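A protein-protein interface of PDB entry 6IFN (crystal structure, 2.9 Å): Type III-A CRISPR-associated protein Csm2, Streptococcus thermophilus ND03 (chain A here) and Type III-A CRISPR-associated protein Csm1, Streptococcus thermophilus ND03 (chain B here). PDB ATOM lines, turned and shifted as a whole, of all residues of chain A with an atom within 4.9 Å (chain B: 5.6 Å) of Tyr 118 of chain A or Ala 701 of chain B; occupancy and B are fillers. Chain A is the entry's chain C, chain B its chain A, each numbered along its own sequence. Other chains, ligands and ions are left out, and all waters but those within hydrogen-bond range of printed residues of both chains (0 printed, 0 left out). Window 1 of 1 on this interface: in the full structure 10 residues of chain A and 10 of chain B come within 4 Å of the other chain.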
ATOM      1  N   VAL A  10     -23.293  22.861  17.070  1.00  0.00           N
ATOM      2  CA  VAL A  10     -23.415  21.594  16.389  1.00  0.00           C
ATOM      3  C   VAL A  10     -24.779  20.989  16.750  1.00  0.00           C
ATOM      4  O   VAL A  10     -25.490  20.522  15.864  1.00  0.00           O
ATOM      5  CB  VAL A  10     -22.229  20.654  16.689  1.00  0.00           C
ATOM      6  CG1 VAL A  10     -22.265  19.408  15.816  1.00  0.00           C
ATOM      7  CG2 VAL A  10     -20.902  21.373  16.515  1.00  0.00           C
ATOM      8  N   GLU A  14     -27.564  19.919  14.039  1.00  0.00           N
ATOM      9  CA  GLU A  14     -28.164  18.604  13.978  1.00  0.00           C
ATOM     10  C   GLU A  14     -29.683  18.762  14.020  1.00  0.00           C
ATOM     11  O   GLU A  14     -30.366  18.214  13.129  1.00  0.00           O
ATOM     12  CB  GLU A  14     -27.673  17.699  15.111  1.00  0.00           C
ATOM     13  CG  GLU A  14     -28.136  16.248  14.980  1.00  0.00           C
ATOM     14  CD  GLU A  14     -27.521  15.300  16.003  1.00  0.00           C
ATOM     15  OE1 GLU A  14     -27.081  15.788  17.061  1.00  0.00           O
ATOM     16  OE2 GLU A  14     -27.462  14.078  15.738  1.00  0.00           O
ATOM     17  N   ILE A  17     -31.063  19.962  10.776  1.00  0.00           N
ATOM     18  CA  ILE A  17     -31.086  18.963   9.729  1.00  0.00           C
ATOM     19  C   ILE A  17     -32.230  17.969   9.986  1.00  0.00           C
ATOM     20  O   ILE A  17     -32.816  17.414   9.058  1.00  0.00           O
ATOM     21  CB  ILE A  17     -29.707  18.297   9.564  1.00  0.00           C
ATOM     22  CG1 ILE A  17     -28.865  19.051   8.535  1.00  0.00           C
ATOM     23  CG2 ILE A  17     -29.822  16.830   9.190  1.00  0.00           C
ATOM     24  CD1 ILE A  17     -28.419  20.397   9.017  1.00  0.00           C
ATOM     25  N   ALA A 114     -21.092  21.795   9.918  1.00  0.00           N
ATOM     26  CA  ALA A 114     -21.837  20.882  10.783  1.00  0.00           C
ATOM     27  C   ALA A 114     -23.164  20.490  10.129  1.00  0.00           C
ATOM     28  O   ALA A 114     -23.509  19.292  10.083  1.00  0.00           O
ATOM     29  CB  ALA A 114     -22.071  21.524  12.128  1.00  0.00           C
ATOM     30  N   LEU A 115     -23.880  21.516   9.641  1.00  0.00           N
ATOM     31  CA  LEU A 115     -25.145  21.346   8.946  1.00  0.00           C
ATOM     32  C   LEU A 115     -24.971  20.291   7.848  1.00  0.00           C
ATOM     33  O   LEU A 115     -25.745  19.351   7.779  1.00  0.00           O
ATOM     34  CB  LEU A 115     -25.594  22.680   8.335  1.00  0.00           C
ATOM     35  CG  LEU A 115     -26.138  23.736   9.296  1.00  0.00           C
ATOM     36  CD1 LEU A 115     -26.357  25.069   8.576  1.00  0.00           C
ATOM     37  CD2 LEU A 115     -27.430  23.272   9.947  1.00  0.00           C
ATOM     38  N   VAL A 116     -23.936  20.466   7.019  1.00  0.00           N
ATOM     39  CA  VAL A 116     -23.723  19.657   5.820  1.00  0.00           C
ATOM     40  C   VAL A 116     -23.393  18.225   6.244  1.00  0.00           C
ATOM     41  O   VAL A 116     -23.884  17.281   5.649  1.00  0.00           O
ATOM     42  CB  VAL A 116     -22.610  20.239   4.927  1.00  0.00           C
ATOM     43  CG1 VAL A 116     -22.253  19.333   3.759  1.00  0.00           C
ATOM     44  CG2 VAL A 116     -22.962  21.630   4.420  1.00  0.00           C
ATOM     45  N   ALA A 117     -22.559  18.083   7.278  1.00  0.00           N
ATOM     46  CA  ALA A 117     -22.157  16.778   7.763  1.00  0.00           C
ATOM     47  C   ALA A 117     -23.398  15.985   8.147  1.00  0.00           C
ATOM     48  O   ALA A 117     -23.588  14.875   7.690  1.00  0.00           O
ATOM     49  CB  ALA A 117     -21.234  16.916   8.940  1.00  0.00           C
ATOM     50  N   TYR A 118     -24.252  16.600   8.965  1.00  0.00           N
ATOM     51  CA  TYR A 118     -25.416  15.909   9.490  1.00  0.00           C
ATOM     52  C   TYR A 118     -26.482  15.749   8.404  1.00  0.00           C
ATOM     53  O   TYR A 118     -27.311  14.862   8.514  1.00  0.00           O
ATOM     54  CB  TYR A 118     -25.955  16.610  10.737  1.00  0.00           C
ATOM     55  CG  TYR A 118     -25.297  16.151  12.008  1.00  0.00           C
ATOM     56  CD1 TYR A 118     -25.316  14.819  12.375  1.00  0.00           C
ATOM     57  CD2 TYR A 118     -24.627  17.039  12.829  1.00  0.00           C
ATOM     58  CE1 TYR A 118     -24.702  14.382  13.536  1.00  0.00           C
ATOM     59  CE2 TYR A 118     -24.019  16.619  13.999  1.00  0.00           C
ATOM     60  CZ  TYR A 118     -24.045  15.282  14.351  1.00  0.00           C
ATOM     61  OH  TYR A 118     -23.414  14.857  15.482  1.00  0.00           O
ATOM     62  N   PHE A 119     -26.446  16.595   7.368  1.00  0.00           N
ATOM     63  CA  PHE A 119     -27.312  16.447   6.188  1.00  0.00           C
ATOM     64  C   PHE A 119     -26.963  15.139   5.477  1.00  0.00           C
ATOM     65  O   PHE A 119     -27.811  14.283   5.289  1.00  0.00           O
ATOM     66  CB  PHE A 119     -27.191  17.655   5.253  1.00  0.00           C
ATOM     67  CG  PHE A 119     -27.762  17.449   3.877  1.00  0.00           C
ATOM     68  CD1 PHE A 119     -29.133  17.422   3.674  1.00  0.00           C
ATOM     69  CD2 PHE A 119     -26.927  17.263   2.790  1.00  0.00           C
ATOM     70  CE1 PHE A 119     -29.653  17.237   2.404  1.00  0.00           C
ATOM     71  CE2 PHE A 119     -27.449  17.069   1.519  1.00  0.00           C
ATOM     72  CZ  PHE A 119     -28.806  17.045   1.331  1.00  0.00           C
ATOM     73  N   LYS A 120     -25.690  14.983   5.122  1.00  0.00           N
ATOM     74  CA  LYS A 120     -25.233  13.795   4.435  1.00  0.00           C
ATOM     75  C   LYS A 120     -25.465  12.560   5.323  1.00  0.00           C
ATOM     76  O   LYS A 120     -25.771  11.472   4.832  1.00  0.00           O
ATOM     77  CB  LYS A 120     -23.760  13.949   4.043  1.00  0.00           C
ATOM     78  CG  LYS A 120     -23.527  14.490   2.642  1.00  0.00           C
ATOM     79  CD  LYS A 120     -23.600  13.408   1.573  1.00  0.00           C
ATOM     80  CE  LYS A 120     -23.139  13.862   0.199  1.00  0.00           C
ATOM     81  NZ  LYS A 120     -23.560  12.909  -0.858  1.00  0.00           N
ATOM     82  N   PHE A 121     -25.297  12.716   6.635  1.00  0.00           N
ATOM     83  CA  PHE A 121     -25.350  11.597   7.533  1.00  0.00           C
ATOM     84  C   PHE A 121     -26.757  11.016   7.534  1.00  0.00           C
ATOM     85  O   PHE A 121     -26.919   9.793   7.469  1.00  0.00           O
ATOM     86  CB  PHE A 121     -24.926  12.012   8.940  1.00  0.00           C
ATOM     87  CG  PHE A 121     -25.042  10.923   9.973  1.00  0.00           C
ATOM     88  CD1 PHE A 121     -24.289   9.765   9.884  1.00  0.00           C
ATOM     89  CD2 PHE A 121     -25.919  11.056  11.031  1.00  0.00           C
ATOM     90  CE1 PHE A 121     -24.400   8.770  10.842  1.00  0.00           C
ATOM     91  CE2 PHE A 121     -26.022  10.065  11.994  1.00  0.00           C
ATOM     92  CZ  PHE A 121     -25.264   8.926  11.895  1.00  0.00           C
ATOM     93  N   TYR A 122     -27.750  11.907   7.622  1.00  0.00           N
ATOM     94  CA  TYR A 122     -29.150  11.523   7.832  1.00  0.00           C
ATOM     95  C   TYR A 122     -29.876  11.334   6.493  1.00  0.00           C
ATOM     96  O   TYR A 122     -31.099  11.458   6.444  1.00  0.00           O
ATOM     97  CB  TYR A 122     -29.875  12.564   8.691  1.00  0.00           C
ATOM     98  CG  TYR A 122     -29.686  12.430  10.182  1.00  0.00           C
ATOM     99  CD1 TYR A 122     -29.892  11.228  10.837  1.00  0.00           C
ATOM    100  CD2 TYR A 122     -29.336  13.525  10.948  1.00  0.00           C
ATOM    101  CE1 TYR A 122     -29.739  11.112  12.205  1.00  0.00           C
ATOM    102  CE2 TYR A 122     -29.159  13.428  12.322  1.00  0.00           C
ATOM    103  CZ  TYR A 122     -29.341  12.208  12.948  1.00  0.00           C
ATOM    104  OH  TYR A 122     -29.175  12.096  14.297  1.00  0.00           O
ATOM    105  N   ARG B 697     -17.267  17.262  20.454  1.00  0.00           N
ATOM    106  CA  ARG B 697     -18.633  17.343  19.922  1.00  0.00           C
ATOM    107  C   ARG B 697     -18.598  17.488  18.391  1.00  0.00           C
ATOM    108  O   ARG B 697     -19.137  16.654  17.699  1.00  0.00           O
ATOM    109  CB  ARG B 697     -19.414  18.498  20.569  1.00  0.00           C
ATOM    110  CG  ARG B 697     -20.925  18.286  20.644  1.00  0.00           C
ATOM    111  CD  ARG B 697     -21.512  17.716  19.361  1.00  0.00           C
ATOM    112  NE  ARG B 697     -22.957  17.561  19.370  1.00  0.00           N
ATOM    113  CZ  ARG B 697     -23.650  16.995  18.386  1.00  0.00           C
ATOM    114  NH1 ARG B 697     -23.019  16.446  17.365  1.00  0.00           N
ATOM    115  NH2 ARG B 697     -24.971  16.988  18.411  1.00  0.00           N
ATOM    116  N   MET B 698     -17.944  18.535  17.880  1.00  0.00           N
ATOM    117  CA  MET B 698     -17.950  18.869  16.442  1.00  0.00           C
ATOM    118  C   MET B 698     -17.350  17.730  15.596  1.00  0.00           C
ATOM    119  O   MET B 698     -17.837  17.407  14.509  1.00  0.00           O
ATOM    120  CB  MET B 698     -17.168  20.164  16.214  1.00  0.00           C
ATOM    121  CG  MET B 698     -16.864  20.440  14.771  1.00  0.00           C
ATOM    122  SD  MET B 698     -18.337  20.821  13.770  1.00  0.00           S
ATOM    123  CE  MET B 698     -17.548  21.867  12.541  1.00  0.00           C
ATOM    124  N   ASN B 699     -16.304  17.090  16.111  1.00  0.00           N
ATOM    125  CA  ASN B 699     -15.693  16.004  15.422  1.00  0.00           C
ATOM    126  C   ASN B 699     -16.628  14.788  15.376  1.00  0.00           C
ATOM    127  O   ASN B 699     -16.316  13.871  14.634  1.00  0.00           O
ATOM    128  CB  ASN B 699     -14.357  15.616  16.042  1.00  0.00           C
ATOM    129  CG  ASN B 699     -13.183  16.350  15.435  1.00  0.00           C
ATOM    130  OD1 ASN B 699     -13.039  16.404  14.218  1.00  0.00           O
ATOM    131  ND2 ASN B 699     -12.303  16.860  16.279  1.00  0.00           N
ATOM    132  N   MET B 700     -17.731  14.760  16.141  1.00  0.00           N
ATOM    133  CA  MET B 700     -18.788  13.764  15.915  1.00  0.00           C
ATOM    134  C   MET B 700     -19.481  14.029  14.573  1.00  0.00           C
ATOM    135  O   MET B 700     -19.836  13.092  13.826  1.00  0.00           O
ATOM    136  CB  MET B 700     -19.864  13.779  16.999  1.00  0.00           C
ATOM    137  CG  MET B 700     -19.334  13.568  18.399  1.00  0.00           C
ATOM    138  SD  MET B 700     -20.677  13.230  19.569  1.00  0.00           S
ATOM    139  CE  MET B 700     -19.888  13.674  21.120  1.00  0.00           C
ATOM    140  N   ALA B 701     -19.671  15.312  14.269  1.00  0.00           N
ATOM    141  CA  ALA B 701     -20.255  15.697  12.999  1.00  0.00           C
ATOM    142  C   ALA B 701     -19.351  15.193  11.869  1.00  0.00           C
ATOM    143  O   ALA B 701     -19.805  14.471  10.957  1.00  0.00           O
ATOM    144  CB  ALA B 701     -20.457  17.194  12.932  1.00  0.00           C
ATOM    145  N   ARG B 702     -18.076  15.580  11.957  1.00  0.00           N
ATOM    146  CA  ARG B 702     -17.095  15.236  10.955  1.00  0.00           C
ATOM    147  C   ARG B 702     -17.021  13.712  10.861  1.00  0.00           C
ATOM    148  O   ARG B 702     -16.944  13.170   9.749  1.00  0.00           O
ATOM    149  CB  ARG B 702     -15.708  15.804  11.272  1.00  0.00           C
ATOM    150  CG  ARG B 702     -15.657  17.313  11.463  1.00  0.00           C
ATOM    151  CD  ARG B 702     -14.271  17.904  11.253  1.00  0.00           C
ATOM    152  NE  ARG B 702     -14.009  19.009  12.170  1.00  0.00           N
ATOM    153  CZ  ARG B 702     -14.152  20.296  11.868  1.00  0.00           C
ATOM    154  NH1 ARG B 702     -14.546  20.651  10.650  1.00  0.00           N
ATOM    155  NH2 ARG B 702     -13.910  21.218  12.785  1.00  0.00           N
ATOM    156  N   LEU B 703     -17.086  13.021  12.007  1.00  0.00           N
ATOM    157  CA  LEU B 703     -17.038  11.569  11.966  1.00  0.00           C
ATOM    158  C   LEU B 703     -18.157  11.036  11.079  1.00  0.00           C
ATOM    159  O   LEU B 703     -17.922  10.176  10.220  1.00  0.00           O
ATOM    160  CB  LEU B 703     -17.215  10.939  13.337  1.00  0.00           C
ATOM    161  CG  LEU B 703     -17.177   9.421  13.242  1.00  0.00           C
ATOM    162  CD1 LEU B 703     -15.804   8.951  12.752  1.00  0.00           C
ATOM    163  CD2 LEU B 703     -17.549   8.772  14.559  1.00  0.00           C
ATOM    164  N   ALA B 704     -19.376  11.526  11.339  1.00  0.00           N
ATOM    165  CA  ALA B 704     -20.536  11.113  10.562  1.00  0.00           C
ATOM    166  C   ALA B 704     -20.292  11.407   9.079  1.00  0.00           C
ATOM    167  O   ALA B 704     -20.575  10.559   8.244  1.00  0.00           O
ATOM    168  CB  ALA B 704     -21.784  11.779  11.064  1.00  0.00           C
ATOM    169  N   TYR B 705     -19.744  12.585   8.759  1.00  0.00           N
ATOM    170  CA  TYR B 705     -19.595  12.963   7.364  1.00  0.00           C
ATOM    171  C   TYR B 705     -18.711  11.948   6.644  1.00  0.00           C
ATOM    172  O   TYR B 705     -19.102  11.422   5.616  1.00  0.00           O
ATOM    173  CB  TYR B 705     -19.015  14.364   7.166  1.00  0.00           C
ATOM    174  CG  TYR B 705     -18.737  14.658   5.713  1.00  0.00           C
ATOM    175  CD1 TYR B 705     -17.541  14.276   5.123  1.00  0.00           C
ATOM    176  CD2 TYR B 705     -19.689  15.257   4.908  1.00  0.00           C
ATOM    177  CE1 TYR B 705     -17.286  14.502   3.779  1.00  0.00           C
ATOM    178  CE2 TYR B 705     -19.444  15.510   3.568  1.00  0.00           C
ATOM    179  CZ  TYR B 705     -18.243  15.122   2.995  1.00  0.00           C
ATOM    180  OH  TYR B 705     -17.991  15.350   1.671  1.00  0.00           O
ATOM    181  N   TYR B 706     -17.507  11.702   7.165  1.00  0.00           N
ATOM    182  CA  TYR B 706     -16.567  10.809   6.475  1.00  0.00           C
ATOM    183  C   TYR B 706     -17.022   9.347   6.600  1.00  0.00           C
ATOM    184  O   TYR B 706     -16.654   8.532   5.776  1.00  0.00           O
ATOM    185  CB  TYR B 706     -15.147  10.941   7.017  1.00  0.00           C
ATOM    186  CG  TYR B 706     -14.541  12.306   6.885  1.00  0.00           C
ATOM    187  CD1 TYR B 706     -13.977  12.732   5.699  1.00  0.00           C
ATOM    188  CD2 TYR B 706     -14.504  13.161   7.964  1.00  0.00           C
ATOM    189  CE1 TYR B 706     -13.408  13.990   5.579  1.00  0.00           C
ATOM    190  CE2 TYR B 706     -13.957  14.425   7.861  1.00  0.00           C
ATOM    191  CZ  TYR B 706     -13.397  14.830   6.670  1.00  0.00           C
ATOM    192  OH  TYR B 706     -12.840  16.065   6.612  1.00  0.00           O
ATOM    193  N   TYR B 730     -20.432   5.182  14.957  1.00  0.00           N
ATOM    194  CA  TYR B 730     -20.879   6.442  15.481  1.00  0.00           C
ATOM    195  C   TYR B 730     -21.447   6.222  16.895  1.00  0.00           C
ATOM    196  O   TYR B 730     -21.337   7.119  17.710  1.00  0.00           O
ATOM    197  CB  TYR B 730     -21.844   7.079  14.477  1.00  0.00           C
ATOM    198  CG  TYR B 730     -22.431   8.415  14.858  1.00  0.00           C
ATOM    199  CD1 TYR B 730     -21.731   9.589  14.666  1.00  0.00           C
ATOM    200  CD2 TYR B 730     -23.714   8.515  15.362  1.00  0.00           C
ATOM    201  CE1 TYR B 730     -22.268  10.827  14.996  1.00  0.00           C
ATOM    202  CE2 TYR B 730     -24.271   9.740  15.691  1.00  0.00           C
ATOM    203  CZ  TYR B 730     -23.551  10.910  15.507  1.00  0.00           C
ATOM    204  OH  TYR B 730     -24.115  12.118  15.842  1.00  0.00           O
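The side-chain carboxylate of Glu 14 of chain A lies within salt-bridge range of the guanidinium group of Arg 697 of chain B (2.8 Å).
The guanidinium group (NH1) of Arg 697 of chain B lies within hydrogen-bond range of the side-chain hydroxyl (OH) of Tyr 118 of chain A, 2.5 Å away.
OH of Tyr 118 of chain A sits at hydrogen-bond distance from OH of Tyr 730 of chain B (2.9 Å).
OH of Tyr 122 of chain A is in hydrogen-bond range of OE2 of Glu 14 of chain A.
Arg 697 of chain B touches Val 10 of chain A.
Val 10 of chain A touches Met 698 of chain B (CG2 to SD, 3.8 Å).
OE2 of Glu 14 of chain A touches OH of Tyr 730 of chain B, at 3.9 Å.
Ala 701 of chain B touches Ala 117 of chain A.
CB of Ala 117 of chain A touches CB of Tyr 705 of chain B, at 3.8 Å.
CB of Ala 701 of chain B touches CE2 of Tyr 118 of chain A, 3.8 Å away.
CD1 of Phe 121 of chain A touches CB of Ala 704 of chain B, at 3.4 Å.
Phe 121 of chain A touches Tyr 730 of chain B (CZ to CD2, 3.8 Å).
Of the printed residues of chain B, Tyr 118 of chain A touches Arg 697, Ala 701 and Tyr 730.
Ala 701 of chain B touches two residues of chain A.
Of the printed residues of chain A, Tyr 705 of chain B touches Ala 117.
Of the printed residues of chain A, Met 698 of chain B touches Val 10.
Of the printed residues of chain B, Glu 14 of chain A touches Arg 697 (2.8 Å) and Tyr 730 (3.9 Å).
Printed residues of chain B within 4 Å of Val 10 of chain A: Arg 697 (3.4 Å) and Met 698 (3.8 Å).
Met 700 of chain B touches none of the printed residues of chain A.
Ile 17 of chain A touches none of the printed residues of chain B.
The nearest residue of chain A that does not touch Ala 701 of chain B is Val 10 of chain A (4.1 Å).
The nearest printed residue of chain A that does not touch Met 698 of chain B is Ala 114 of chain A (4.1 Å).
Hydrophobic or aromatic side chains of chain B within 4 Å of the printed part of chain A: Met 698, Ala 701, Ala 704, Tyr 705 and Tyr 730.
Of the 12 printed residues of chain A, 5 touch a printed residue of chain B.
Among the printed residues, 11 pairs touch across the chains.
Among the printed residues, Asp or Glu carboxylates within 4 Å of a Lys or Arg side-chain nitrogen of the other chain: Glu 14 of chain A with Arg 697 of chain B (2.8 Å).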
